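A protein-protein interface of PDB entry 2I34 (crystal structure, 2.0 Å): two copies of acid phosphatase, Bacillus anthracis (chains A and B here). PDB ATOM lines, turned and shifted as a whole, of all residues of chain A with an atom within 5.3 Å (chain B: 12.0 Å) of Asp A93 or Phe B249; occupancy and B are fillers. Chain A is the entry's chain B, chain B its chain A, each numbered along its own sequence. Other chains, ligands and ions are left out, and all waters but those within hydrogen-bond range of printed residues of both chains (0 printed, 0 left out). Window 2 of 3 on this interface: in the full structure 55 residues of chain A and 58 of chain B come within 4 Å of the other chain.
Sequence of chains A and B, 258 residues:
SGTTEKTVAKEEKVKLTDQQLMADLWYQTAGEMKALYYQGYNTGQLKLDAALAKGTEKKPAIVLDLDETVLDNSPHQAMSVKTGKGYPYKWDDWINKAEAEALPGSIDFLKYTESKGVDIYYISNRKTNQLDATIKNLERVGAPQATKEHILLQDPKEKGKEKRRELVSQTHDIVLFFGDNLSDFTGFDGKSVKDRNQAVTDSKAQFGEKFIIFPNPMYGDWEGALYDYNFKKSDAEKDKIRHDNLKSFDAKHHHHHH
CA of Pro A75 touches O of Lys B247 (3.2 Å). CA of Ser B248 touches O of Pro A75 (3.7 Å). O of Phe B249 touches CG of Met A79 (3.3 Å). Lys A90 touches Phe B249. OD1 of Asp A93 touches CZ of Phe B249 (3.4 Å). CE3 of Trp A94 touches CG of Phe B249, at 3.5 Å.
Of the 8 printed residues of chain B, 3 touch a printed residue of chain A.
No position is printed for both chains. Of the 7 pairs that touch across the chains among the printed residues, none has its exchanged pair printed and touching as well.
The backbone NH (N) of Phe B249 is in hydrogen-bond range of the backbone carbonyl oxygen (O) of Pro A75 (3.0 Å).
Printed residues of chain B within 4 Å of Pro A75: Lys B247 (3.2 Å), Ser B248 (3.7 Å) and Phe B249 (3.0 Å). No residue of chain B comes within 4 Å of His A76. Of the printed residues of chain B, Met A79 touches Phe B249. Printed residues of chain B within 4 Å of Lys A90: Phe B249 (3.9 Å). No residue of chain B comes within 4 Å of Asp A92. Of chain B, only Phe B249 comes within 4 Å of Asp A93. Of chain B, only Phe B249 comes within 4 Å of Trp A94. Asn A96 touches none of the printed residues of chain B. No residue of chain B comes within 4 Å of Lys A97. Asn B245 touches none of the printed residues of chain A. Printed residues of chain A within 4 Å of Lys B247: Pro A75. Printed residues of chain A within 4 Å of Ser B248: Pro A75 (3.7 Å). Phe B249 touches just these residues of chain A: Pro A75, Met A79, Lys A90, Asp A93 and Trp A94. The nearest residue of chain B that does not touch Asp A93 is Asp B250 (5.8 Å). The nearest residue of chain A that does not touch Phe B249 is His A76 (4.02 Å). The nearest printed residue of chain B that does not touch Met A79 is Ser B248 (4.0003 Å).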
ATOM      1  N   PRO A  75      25.153  -6.981  -3.318  1.00  0.00           N
ATOM      2  CA  PRO A  75      24.006  -7.881  -3.196  1.00  0.00           C
ATOM      3  C   PRO A  75      23.501  -8.113  -1.767  1.00  0.00           C
ATOM      4  O   PRO A  75      22.293  -8.258  -1.568  1.00  0.00           O
ATOM      5  CB  PRO A  75      24.516  -9.176  -3.835  1.00  0.00           C
ATOM      6  CG  PRO A  75      25.540  -8.695  -4.841  1.00  0.00           C
ATOM      7  CD  PRO A  75      26.247  -7.616  -4.086  1.00  0.00           C
ATOM      8  N   HIS A  76      24.394  -8.132  -0.783  1.00  0.00           N
ATOM      9  CA  HIS A  76      23.947  -8.227   0.599  1.00  0.00           C
ATOM     10  C   HIS A  76      23.225  -6.937   0.993  1.00  0.00           C
ATOM     11  O   HIS A  76      22.171  -6.970   1.630  1.00  0.00           O
ATOM     12  CB  HIS A  76      25.108  -8.494   1.563  1.00  0.00           C
ATOM     13  CG  HIS A  76      24.697  -8.455   2.996  1.00  0.00           C
ATOM     14  ND1 HIS A  76      24.600  -7.276   3.706  1.00  0.00           N
ATOM     15  CD2 HIS A  76      24.304  -9.437   3.836  1.00  0.00           C
ATOM     16  CE1 HIS A  76      24.197  -7.543   4.935  1.00  0.00           C
ATOM     17  NE2 HIS A  76      24.001  -8.845   5.037  1.00  0.00           N
ATOM     18  N   MET A  79      19.833  -6.847  -0.417  1.00  0.00           N
ATOM     19  CA  MET A  79      19.005  -7.740   0.375  1.00  0.00           C
ATOM     20  C   MET A  79      18.465  -7.036   1.640  1.00  0.00           C
ATOM     21  O   MET A  79      17.295  -7.187   1.974  1.00  0.00           O
ATOM     22  CB  MET A  79      19.806  -9.003   0.719  1.00  0.00           C
ATOM     23  CG  MET A  79      19.065 -10.050   1.543  1.00  0.00           C
ATOM     24  SD  MET A  79      19.124  -9.715   3.310  1.00  0.00           S
ATOM     25  CE  MET A  79      20.881  -9.521   3.626  1.00  0.00           C
ATOM     26  N   LYS A  90      22.212 -11.617   8.039  1.00  0.00           N
ATOM     27  CA  LYS A  90      22.791 -12.423   6.938  1.00  0.00           C
ATOM     28  C   LYS A  90      24.189 -12.031   6.434  1.00  0.00           C
ATOM     29  O   LYS A  90      24.621 -12.501   5.369  1.00  0.00           O
ATOM     30  CB  LYS A  90      21.807 -12.513   5.759  1.00  0.00           C
ATOM     31  CG  LYS A  90      20.521 -13.261   6.064  1.00  0.00           C
ATOM     32  CD  LYS A  90      20.773 -14.730   6.223  1.00  0.00           C
ATOM     33  CE  LYS A  90      19.503 -15.507   6.473  1.00  0.00           C
ATOM     34  NZ  LYS A  90      19.777 -16.590   7.439  1.00  0.00           N
ATOM     35  N   TRP A  91      24.917 -11.187   7.174  1.00  0.00           N
ATOM     36  CA  TRP A  91      26.249 -10.765   6.710  1.00  0.00           C
ATOM     37  C   TRP A  91      27.260 -11.924   6.714  1.00  0.00           C
ATOM     38  O   TRP A  91      27.919 -12.188   5.708  1.00  0.00           O
ATOM     39  CB  TRP A  91      26.791  -9.586   7.528  1.00  0.00           C
ATOM     40  CG  TRP A  91      28.172  -9.193   7.122  1.00  0.00           C
ATOM     41  CD1 TRP A  91      29.327  -9.475   7.789  1.00  0.00           C
ATOM     42  CD2 TRP A  91      28.559  -8.485   5.932  1.00  0.00           C
ATOM     43  NE1 TRP A  91      30.404  -8.979   7.100  1.00  0.00           N
ATOM     44  CE2 TRP A  91      29.962  -8.369   5.955  1.00  0.00           C
ATOM     45  CE3 TRP A  91      27.858  -7.941   4.854  1.00  0.00           C
ATOM     46  CZ2 TRP A  91      30.679  -7.715   4.947  1.00  0.00           C
ATOM     47  CZ3 TRP A  91      28.570  -7.294   3.852  1.00  0.00           C
ATOM     48  CH2 TRP A  91      29.968  -7.186   3.909  1.00  0.00           C
ATOM     49  N   ASP A  92      27.372 -12.615   7.845  1.00  0.00           N
ATOM     50  CA  ASP A  92      28.285 -13.758   7.959  1.00  0.00           C
ATOM     51  C   ASP A  92      27.940 -14.886   6.970  1.00  0.00           C
ATOM     52  O   ASP A  92      28.830 -15.551   6.435  1.00  0.00           O
ATOM     53  CB  ASP A  92      28.267 -14.302   9.394  1.00  0.00           C
ATOM     54  CG  ASP A  92      28.850 -13.318  10.394  1.00  0.00           C
ATOM     55  OD1 ASP A  92      29.440 -12.303   9.968  1.00  0.00           O
ATOM     56  OD2 ASP A  92      28.711 -13.557  11.605  1.00  0.00           O
ATOM     57  N   ASP A  93      26.645 -15.095   6.745  1.00  0.00           N
ATOM     58  CA  ASP A  93      26.166 -16.064   5.760  1.00  0.00           C
ATOM     59  C   ASP A  93      26.639 -15.675   4.352  1.00  0.00           C
ATOM     60  O   ASP A  93      27.160 -16.507   3.616  1.00  0.00           O
ATOM     61  CB  ASP A  93      24.635 -16.152   5.825  1.00  0.00           C
ATOM     62  CG  ASP A  93      24.087 -17.331   5.065  1.00  0.00           C
ATOM     63  OD1 ASP A  93      23.673 -17.133   3.905  1.00  0.00           O
ATOM     64  OD2 ASP A  93      24.088 -18.458   5.610  1.00  0.00           O
ATOM     65  N   TRP A  94      26.463 -14.403   4.002  1.00  0.00           N
ATOM     66  CA  TRP A  94      26.969 -13.834   2.748  1.00  0.00           C
ATOM     67  C   TRP A  94      28.480 -14.003   2.582  1.00  0.00           C
ATOM     68  O   TRP A  94      28.950 -14.391   1.516  1.00  0.00           O
ATOM     69  CB  TRP A  94      26.605 -12.345   2.643  1.00  0.00           C
ATOM     70  CG  TRP A  94      27.375 -11.608   1.569  1.00  0.00           C
ATOM     71  CD1 TRP A  94      28.412 -10.753   1.752  1.00  0.00           C
ATOM     72  CD2 TRP A  94      27.181 -11.712   0.157  1.00  0.00           C
ATOM     73  NE1 TRP A  94      28.872 -10.295   0.540  1.00  0.00           N
ATOM     74  CE2 TRP A  94      28.139 -10.873  -0.459  1.00  0.00           C
ATOM     75  CE3 TRP A  94      26.292 -12.433  -0.649  1.00  0.00           C
ATOM     76  CZ2 TRP A  94      28.235 -10.733  -1.854  1.00  0.00           C
ATOM     77  CZ3 TRP A  94      26.384 -12.290  -2.038  1.00  0.00           C
ATOM     78  CH2 TRP A  94      27.346 -11.432  -2.621  1.00  0.00           C
ATOM     79  N   ILE A  95      29.231 -13.685   3.632  1.00  0.00           N
ATOM     80  CA  ILE A  95      30.685 -13.872   3.624  1.00  0.00           C
ATOM     81  C   ILE A  95      31.038 -15.339   3.360  1.00  0.00           C
ATOM     82  O   ILE A  95      31.858 -15.627   2.488  1.00  0.00           O
ATOM     83  CB  ILE A  95      31.348 -13.379   4.965  1.00  0.00           C
ATOM     84  CG1 ILE A  95      31.230 -11.856   5.123  1.00  0.00           C
ATOM     85  CG2 ILE A  95      32.812 -13.815   5.065  1.00  0.00           C
ATOM     86  CD1 ILE A  95      31.927 -11.014   4.069  1.00  0.00           C
ATOM     87  N   ASN A  96      30.399 -16.255   4.090  1.00  0.00           N
ATOM     88  CA  ASN A  96      30.672 -17.686   3.962  1.00  0.00           C
ATOM     89  C   ASN A  96      30.317 -18.257   2.582  1.00  0.00           C
ATOM     90  O   ASN A  96      30.927 -19.217   2.122  1.00  0.00           O
ATOM     91  CB  ASN A  96      29.919 -18.461   5.049  1.00  0.00           C
ATOM     92  CG  ASN A  96      30.618 -19.728   5.443  1.00  0.00           C
ATOM     93  OD1 ASN A  96      31.818 -19.724   5.725  1.00  0.00           O
ATOM     94  ND2 ASN A  96      29.873 -20.828   5.481  1.00  0.00           N
ATOM     95  N   LYS A  97      29.326 -17.661   1.925  1.00  0.00           N
ATOM     96  CA  LYS A  97      28.954 -18.067   0.567  1.00  0.00           C
ATOM     97  C   LYS A  97      30.119 -17.831  -0.415  1.00  0.00           C
ATOM     98  O   LYS A  97      30.250 -18.554  -1.403  1.00  0.00           O
ATOM     99  CB  LYS A  97      27.704 -17.315   0.095  1.00  0.00           C
ATOM    100  N   GLU A  99      30.869 -15.641  -2.710  1.00  0.00           N
ATOM    101  CA  GLU A  99      30.398 -15.465  -4.088  1.00  0.00           C
ATOM    102  C   GLU A  99      30.334 -13.993  -4.513  1.00  0.00           C
ATOM    103  O   GLU A  99      29.655 -13.650  -5.486  1.00  0.00           O
ATOM    104  CB  GLU A  99      29.036 -16.154  -4.266  1.00  0.00           C
ATOM    105  CG  GLU A  99      27.939 -15.636  -3.335  1.00  0.00           C
ATOM    106  CD  GLU A  99      26.627 -16.378  -3.486  1.00  0.00           C
ATOM    107  OE1 GLU A  99      26.583 -17.585  -3.170  1.00  0.00           O
ATOM    108  OE2 GLU A  99      25.632 -15.738  -3.908  1.00  0.00           O
ATOM    109  N   HIS B 243      13.103  -0.802  -6.837  1.00  0.00           N
ATOM    110  CA  HIS B 243      13.168  -2.103  -6.169  1.00  0.00           C
ATOM    111  C   HIS B 243      13.488  -3.272  -7.111  1.00  0.00           C
ATOM    112  O   HIS B 243      14.306  -4.138  -6.773  1.00  0.00           O
ATOM    113  CB  HIS B 243      11.861  -2.389  -5.408  1.00  0.00           C
ATOM    114  CG  HIS B 243      11.777  -1.693  -4.085  1.00  0.00           C
ATOM    115  ND1 HIS B 243      11.257  -0.424  -3.940  1.00  0.00           N
ATOM    116  CD2 HIS B 243      12.167  -2.084  -2.847  1.00  0.00           C
ATOM    117  CE1 HIS B 243      11.313  -0.074  -2.665  1.00  0.00           C
ATOM    118  NE2 HIS B 243      11.863  -1.061  -1.983  1.00  0.00           N
ATOM    119  N   ASP B 244      12.868  -3.291  -8.289  1.00  0.00           N
ATOM    120  CA  ASP B 244      13.088  -4.381  -9.247  1.00  0.00           C
ATOM    121  C   ASP B 244      14.511  -4.437  -9.806  1.00  0.00           C
ATOM    122  O   ASP B 244      14.948  -5.497 -10.241  1.00  0.00           O
ATOM    123  CB  ASP B 244      12.090  -4.316 -10.413  1.00  0.00           C
ATOM    124  CG  ASP B 244      10.661  -4.653  -9.999  1.00  0.00           C
ATOM    125  OD1 ASP B 244      10.438  -5.180  -8.886  1.00  0.00           O
ATOM    126  OD2 ASP B 244       9.752  -4.397 -10.812  1.00  0.00           O
ATOM    127  N   ASN B 245      15.236  -3.321  -9.788  1.00  0.00           N
ATOM    128  CA  ASN B 245      16.581  -3.279 -10.368  1.00  0.00           C
ATOM    129  C   ASN B 245      17.706  -3.461  -9.352  1.00  0.00           C
ATOM    130  O   ASN B 245      18.865  -3.535  -9.727  1.00  0.00           O
ATOM    131  CB  ASN B 245      16.773  -2.021 -11.232  1.00  0.00           C
ATOM    132  CG  ASN B 245      16.067  -2.146 -12.591  1.00  0.00           C
ATOM    133  OD1 ASN B 245      16.662  -2.612 -13.564  1.00  0.00           O
ATOM    134  ND2 ASN B 245      14.779  -1.791 -12.640  1.00  0.00           N
ATOM    135  N   LEU B 246      17.364  -3.568  -8.076  1.00  0.00           N
ATOM    136  CA  LEU B 246      18.299  -4.115  -7.099  1.00  0.00           C
ATOM    137  C   LEU B 246      18.622  -5.569  -7.436  1.00  0.00           C
ATOM    138  O   LEU B 246      17.777  -6.294  -7.957  1.00  0.00           O
ATOM    139  CB  LEU B 246      17.723  -4.047  -5.692  1.00  0.00           C
ATOM    140  CG  LEU B 246      17.582  -2.651  -5.103  1.00  0.00           C
ATOM    141  CD1 LEU B 246      16.771  -2.737  -3.826  1.00  0.00           C
ATOM    142  CD2 LEU B 246      18.951  -2.007  -4.869  1.00  0.00           C
ATOM    143  N   LYS B 247      19.851  -5.983  -7.142  1.00  0.00           N
ATOM    144  CA  LYS B 247      20.294  -7.367  -7.339  1.00  0.00           C
ATOM    145  C   LYS B 247      20.588  -7.958  -5.976  1.00  0.00           C
ATOM    146  O   LYS B 247      21.705  -7.852  -5.470  1.00  0.00           O
ATOM    147  CB  LYS B 247      21.548  -7.422  -8.210  1.00  0.00           C
ATOM    148  CG  LYS B 247      21.342  -6.942  -9.634  1.00  0.00           C
ATOM    149  N   SER B 248      19.580  -8.608  -5.405  1.00  0.00           N
ATOM    150  CA  SER B 248      19.652  -9.079  -4.030  1.00  0.00           C
ATOM    151  C   SER B 248      20.245 -10.487  -3.910  1.00  0.00           C
ATOM    152  O   SER B 248      20.049 -11.338  -4.770  1.00  0.00           O
ATOM    153  CB  SER B 248      18.264  -9.029  -3.380  1.00  0.00           C
ATOM    154  OG  SER B 248      17.270  -9.554  -4.245  1.00  0.00           O
ATOM    155  N   PHE B 249      20.972 -10.688  -2.818  1.00  0.00           N
ATOM    156  CA  PHE B 249      21.469 -11.972  -2.371  1.00  0.00           C
ATOM    157  C   PHE B 249      20.286 -12.732  -1.741  1.00  0.00           C
ATOM    158  O   PHE B 249      19.537 -12.151  -0.944  1.00  0.00           O
ATOM    159  CB  PHE B 249      22.583 -11.680  -1.347  1.00  0.00           C
ATOM    160  CG  PHE B 249      22.866 -12.784  -0.388  1.00  0.00           C
ATOM    161  CD1 PHE B 249      23.218 -14.050  -0.842  1.00  0.00           C
ATOM    162  CD2 PHE B 249      22.842 -12.543   0.980  1.00  0.00           C
ATOM    163  CE1 PHE B 249      23.511 -15.068   0.047  1.00  0.00           C
ATOM    164  CE2 PHE B 249      23.132 -13.555   1.878  1.00  0.00           C
ATOM    165  CZ  PHE B 249      23.467 -14.829   1.409  1.00  0.00           C
ATOM    166  N   ASP B 250      20.110 -14.001  -2.110  1.00  0.00           N
ATOM    167  CA  ASP B 250      19.039 -14.843  -1.555  1.00  0.00           C
ATOM    168  C   ASP B 250      19.592 -15.760  -0.461  1.00  0.00           C
ATOM    169  O   ASP B 250      20.272 -16.750  -0.754  1.00  0.00           O
ATOM    170  CB  ASP B 250      18.376 -15.675  -2.666  1.00  0.00           C
ATOM    171  CG  ASP B 250      17.188 -16.511  -2.166  1.00  0.00           C
ATOM    172  OD1 ASP B 250      17.332 -17.278  -1.188  1.00  0.00           O
ATOM    173  OD2 ASP B 250      16.108 -16.426  -2.785  1.00  0.00           O
